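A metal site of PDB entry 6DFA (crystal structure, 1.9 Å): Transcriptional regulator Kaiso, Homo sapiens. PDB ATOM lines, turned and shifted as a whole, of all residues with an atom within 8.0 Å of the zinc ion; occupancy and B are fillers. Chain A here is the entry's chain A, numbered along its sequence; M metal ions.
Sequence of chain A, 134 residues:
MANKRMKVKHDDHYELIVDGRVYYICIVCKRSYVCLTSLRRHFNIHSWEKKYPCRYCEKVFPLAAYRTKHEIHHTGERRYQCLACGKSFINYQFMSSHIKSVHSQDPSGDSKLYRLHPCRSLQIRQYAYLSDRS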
ATOM      1  N   PRO A  53     -24.178   0.796   7.628  1.00  0.00           N
ATOM      2  CA  PRO A  53     -24.264   2.057   6.882  1.00  0.00           C
ATOM      3  C   PRO A  53     -24.436   3.254   7.816  1.00  0.00           C
ATOM      4  O   PRO A  53     -25.255   3.176   8.733  1.00  0.00           O
ATOM      5  CB  PRO A  53     -25.511   1.874   6.018  1.00  0.00           C
ATOM      6  CG  PRO A  53     -26.367   0.928   6.801  1.00  0.00           C
ATOM      7  CD  PRO A  53     -25.416   0.007   7.517  1.00  0.00           C
ATOM      8  N   CYS A  54     -23.640   4.304   7.596  1.00  0.00           N
ATOM      9  CA  CYS A  54     -23.792   5.567   8.319  1.00  0.00           C
ATOM     10  C   CYS A  54     -25.237   6.022   8.154  1.00  0.00           C
ATOM     11  O   CYS A  54     -25.785   5.964   7.050  1.00  0.00           O
ATOM     12  CB  CYS A  54     -22.805   6.609   7.785  1.00  0.00           C
ATOM     13  SG  CYS A  54     -22.998   8.338   8.403  1.00  0.00           S
ATOM     14  N   ARG A  55     -25.893   6.450   9.233  1.00  0.00           N
ATOM     15  CA  ARG A  55     -27.293   6.881   9.072  1.00  0.00           C
ATOM     16  C   ARG A  55     -27.374   8.334   8.585  1.00  0.00           C
ATOM     17  O   ARG A  55     -28.471   8.860   8.404  1.00  0.00           O
ATOM     18  CB  ARG A  55     -28.088   6.716  10.376  1.00  0.00           C
ATOM     19  CG  ARG A  55     -27.885   7.824  11.419  1.00  0.00           C
ATOM     20  CD  ARG A  55     -29.023   7.857  12.440  1.00  0.00           C
ATOM     21  NE  ARG A  55     -30.187   8.602  11.956  1.00  0.00           N
ATOM     22  CZ  ARG A  55     -31.271   8.875  12.680  1.00  0.00           C
ATOM     23  NH1 ARG A  55     -31.358   8.470  13.933  1.00  0.00           N
ATOM     24  NH2 ARG A  55     -32.272   9.558  12.137  1.00  0.00           N
ATOM     25  N   TYR A  56     -26.228   8.968   8.354  1.00  0.00           N
ATOM     26  CA  TYR A  56     -26.250  10.375   7.953  1.00  0.00           C
ATOM     27  C   TYR A  56     -25.691  10.601   6.568  1.00  0.00           C
ATOM     28  O   TYR A  56     -25.869  11.659   5.987  1.00  0.00           O
ATOM     29  CB  TYR A  56     -25.458  11.236   8.937  1.00  0.00           C
ATOM     30  CG  TYR A  56     -25.964  11.175  10.343  1.00  0.00           C
ATOM     31  CD1 TYR A  56     -27.097  11.877  10.733  1.00  0.00           C
ATOM     32  CD2 TYR A  56     -25.332  10.379  11.284  1.00  0.00           C
ATOM     33  CE1 TYR A  56     -27.564  11.806  12.034  1.00  0.00           C
ATOM     34  CE2 TYR A  56     -25.778  10.308  12.573  1.00  0.00           C
ATOM     35  CZ  TYR A  56     -26.893  11.015  12.938  1.00  0.00           C
ATOM     36  OH  TYR A  56     -27.328  10.917  14.245  1.00  0.00           O
ATOM     37  N   CYS A  57     -25.009   9.596   6.033  1.00  0.00           N
ATOM     38  CA  CYS A  57     -24.459   9.722   4.689  1.00  0.00           C
ATOM     39  C   CYS A  57     -24.334   8.335   4.048  1.00  0.00           C
ATOM     40  O   CYS A  57     -24.864   7.354   4.585  1.00  0.00           O
ATOM     41  CB  CYS A  57     -23.108  10.441   4.726  1.00  0.00           C
ATOM     42  SG  CYS A  57     -21.685   9.436   5.146  1.00  0.00           S
ATOM     43  N   GLU A  58     -23.628   8.271   2.921  1.00  0.00           N
ATOM     44  CA  GLU A  58     -23.597   7.090   2.063  1.00  0.00           C
ATOM     45  C   GLU A  58     -22.554   6.062   2.494  1.00  0.00           C
ATOM     46  O   GLU A  58     -22.563   4.941   1.984  1.00  0.00           O
ATOM     47  CB  GLU A  58     -23.336   7.501   0.605  1.00  0.00           C
ATOM     48  CG  GLU A  58     -21.968   8.185   0.277  1.00  0.00           C
ATOM     49  CD  GLU A  58     -21.732   9.549   0.948  1.00  0.00           C
ATOM     50  OE1 GLU A  58     -22.422   9.892   1.916  1.00  0.00           O
ATOM     51  OE2 GLU A  58     -20.830  10.279   0.497  1.00  0.00           O
ATOM     52  N   LYS A  59     -21.668   6.427   3.405  1.00  0.00           N
ATOM     53  CA  LYS A  59     -20.563   5.531   3.758  1.00  0.00           C
ATOM     54  C   LYS A  59     -21.070   4.271   4.453  1.00  0.00           C
ATOM     55  O   LYS A  59     -22.072   4.288   5.168  1.00  0.00           O
ATOM     56  CB  LYS A  59     -19.539   6.245   4.636  1.00  0.00           C
ATOM     57  CG  LYS A  59     -18.656   7.230   3.885  1.00  0.00           C
ATOM     58  CD  LYS A  59     -17.530   7.749   4.782  1.00  0.00           C
ATOM     59  CE  LYS A  59     -16.892   9.015   4.232  1.00  0.00           C
ATOM     60  NZ  LYS A  59     -17.857  10.162   4.193  1.00  0.00           N
ATOM     61  N   VAL A  60     -20.373   3.162   4.215  1.00  0.00           N
ATOM     62  CA  VAL A  60     -20.719   1.881   4.805  1.00  0.00           C
ATOM     63  C   VAL A  60     -19.471   1.263   5.437  1.00  0.00           C
ATOM     64  O   VAL A  60     -18.397   1.313   4.848  1.00  0.00           O
ATOM     65  CB  VAL A  60     -21.299   0.926   3.763  1.00  0.00           C
ATOM     66  CG1 VAL A  60     -21.658  -0.414   4.403  1.00  0.00           C
ATOM     67  CG2 VAL A  60     -22.502   1.554   3.087  1.00  0.00           C
ATOM     68  N   PHE A  61     -19.622   0.696   6.633  1.00  0.00           N
ATOM     69  CA  PHE A  61     -18.501   0.133   7.389  1.00  0.00           C
ATOM     70  C   PHE A  61     -18.653  -1.378   7.633  1.00  0.00           C
ATOM     71  O   PHE A  61     -19.770  -1.868   7.712  1.00  0.00           O
ATOM     72  CB  PHE A  61     -18.353   0.867   8.725  1.00  0.00           C
ATOM     73  CG  PHE A  61     -18.112   2.334   8.561  1.00  0.00           C
ATOM     74  CD1 PHE A  61     -16.818   2.835   8.495  1.00  0.00           C
ATOM     75  CD2 PHE A  61     -19.169   3.216   8.448  1.00  0.00           C
ATOM     76  CE1 PHE A  61     -16.595   4.191   8.315  1.00  0.00           C
ATOM     77  CE2 PHE A  61     -18.954   4.576   8.279  1.00  0.00           C
ATOM     78  CZ  PHE A  61     -17.663   5.063   8.215  1.00  0.00           C
ATOM     79  N   ARG A  67     -18.539   2.410  12.315  1.00  0.00           N
ATOM     80  CA  ARG A  67     -19.660   3.266  11.966  1.00  0.00           C
ATOM     81  C   ARG A  67     -20.001   4.274  13.086  1.00  0.00           C
ATOM     82  O   ARG A  67     -20.243   5.456  12.822  1.00  0.00           O
ATOM     83  CB  ARG A  67     -20.893   2.444  11.625  1.00  0.00           C
ATOM     84  CG  ARG A  67     -22.118   3.375  11.473  1.00  0.00           C
ATOM     85  CD  ARG A  67     -23.353   2.621  11.105  1.00  0.00           C
ATOM     86  NE  ARG A  67     -23.704   1.659  12.144  1.00  0.00           N
ATOM     87  CZ  ARG A  67     -24.767   0.878  12.099  1.00  0.00           C
ATOM     88  NH1 ARG A  67     -25.585   0.960  11.069  1.00  0.00           N
ATOM     89  NH2 ARG A  67     -24.999   0.020  13.084  1.00  0.00           N
ATOM     90  N   HIS A  70     -17.571   7.099  13.306  1.00  0.00           N
ATOM     91  CA  HIS A  70     -17.833   7.966  12.167  1.00  0.00           C
ATOM     92  C   HIS A  70     -19.027   8.881  12.397  1.00  0.00           C
ATOM     93  O   HIS A  70     -18.978  10.077  12.108  1.00  0.00           O
ATOM     94  CB  HIS A  70     -18.069   7.135  10.914  1.00  0.00           C
ATOM     95  CG  HIS A  70     -18.561   7.929   9.764  1.00  0.00           C
ATOM     96  ND1 HIS A  70     -17.746   8.761   9.031  1.00  0.00           N
ATOM     97  CD2 HIS A  70     -19.801   8.037   9.213  1.00  0.00           C
ATOM     98  CE1 HIS A  70     -18.456   9.331   8.066  1.00  0.00           C
ATOM     99  NE2 HIS A  70     -19.696   8.896   8.147  1.00  0.00           N
ATOM    100  N   GLU A  71     -20.121   8.320  12.901  1.00  0.00           N
ATOM    101  CA  GLU A  71     -21.347   9.075  13.114  1.00  0.00           C
ATOM    102  C   GLU A  71     -21.164  10.189  14.133  1.00  0.00           C
ATOM    103  O   GLU A  71     -21.801  11.234  14.047  1.00  0.00           O
ATOM    104  CB  GLU A  71     -22.482   8.130  13.516  1.00  0.00           C
ATOM    105  CG  GLU A  71     -22.932   7.223  12.348  1.00  0.00           C
ATOM    106  CD  GLU A  71     -24.134   6.349  12.676  1.00  0.00           C
ATOM    107  OE1 GLU A  71     -24.322   6.006  13.851  1.00  0.00           O
ATOM    108  OE2 GLU A  71     -24.899   6.041  11.738  1.00  0.00           O
ATOM    109  N   ILE A  72     -20.276   9.966  15.094  1.00  0.00           N
ATOM    110  CA  ILE A  72     -19.953  11.003  16.068  1.00  0.00           C
ATOM    111  C   ILE A  72     -19.437  12.262  15.379  1.00  0.00           C
ATOM    112  O   ILE A  72     -19.731  13.377  15.812  1.00  0.00           O
ATOM    113  CB  ILE A  72     -18.929  10.497  17.115  1.00  0.00           C
ATOM    114  CG1 ILE A  72     -19.639   9.626  18.128  1.00  0.00           C
ATOM    115  CG2 ILE A  72     -18.251  11.664  17.848  1.00  0.00           C
ATOM    116  CD1 ILE A  72     -20.538  10.416  19.051  1.00  0.00           C
ATOM    117  N   HIS A  73     -18.677  12.106  14.291  1.00  0.00           N
ATOM    118  CA  HIS A  73     -18.233  13.259  13.491  1.00  0.00           C
ATOM    119  C   HIS A  73     -19.390  14.067  12.898  1.00  0.00           C
ATOM    120  O   HIS A  73     -19.299  15.289  12.756  1.00  0.00           O
ATOM    121  CB  HIS A  73     -17.311  12.799  12.350  1.00  0.00           C
ATOM    122  CG  HIS A  73     -15.878  12.631  12.753  1.00  0.00           C
ATOM    123  ND1 HIS A  73     -15.410  11.491  13.371  1.00  0.00           N
ATOM    124  CD2 HIS A  73     -14.816  13.460  12.615  1.00  0.00           C
ATOM    125  CE1 HIS A  73     -14.114  11.631  13.605  1.00  0.00           C
ATOM    126  NE2 HIS A  73     -13.728  12.803  13.157  1.00  0.00           N
ATOM    127  N   HIS A  74     -20.451  13.385  12.481  1.00  0.00           N
ATOM    128  CA  HIS A  74     -21.640  14.090  11.995  1.00  0.00           C
ATOM    129  C   HIS A  74     -22.285  14.947  13.083  1.00  0.00           C
ATOM    130  O   HIS A  74     -22.693  16.091  12.825  1.00  0.00           O
ATOM    131  CB  HIS A  74     -22.658  13.081  11.451  1.00  0.00           C
ATOM    132  CG  HIS A  74     -22.328  12.547  10.099  1.00  0.00           C
ATOM    133  ND1 HIS A  74     -22.384  13.335   8.962  1.00  0.00           N
ATOM    134  CD2 HIS A  74     -21.968  11.302   9.671  1.00  0.00           C
ATOM    135  CE1 HIS A  74     -22.066  12.597   7.905  1.00  0.00           C
ATOM    136  NE2 HIS A  74     -21.804  11.370   8.310  1.00  0.00           N
HETATM  137 ZN    ZN M   1     -21.511   9.538   7.429  1.00  0.00          ZN
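SG of Cys 54 lies close to N of Tyr 56 (3.3 Å).
The backbone carbonyl oxygen (O) of Lys 59 is in hydrogen-bond range of the backbone NH (N) of Cys 54.
The backbone NH (N) of Lys 59 lies close to the side-chain sulfur (SG) of Cys 57.
OE1 of Glu 58 sits close to SG of Cys 57, 3.3 Å away.
Along chain A the residues within 4 Å of the zinc ion span positions 54 to 74.
The nearest printed residue that does not touch the zinc ion is Tyr 56 (4.4 Å).
The zinc ion is bound by NE2 of His 74 (2.1 Å).
The zinc ion is bound by a ring nitrogen (NE2) of His 70 (2.1 Å).
SG of Cys 54 binds the zinc ion, 2.1 Å away.
SG of Cys 57 is bound to the zinc ion, at 2.3 Å.
The zinc ion has four donor atoms within binding distance.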
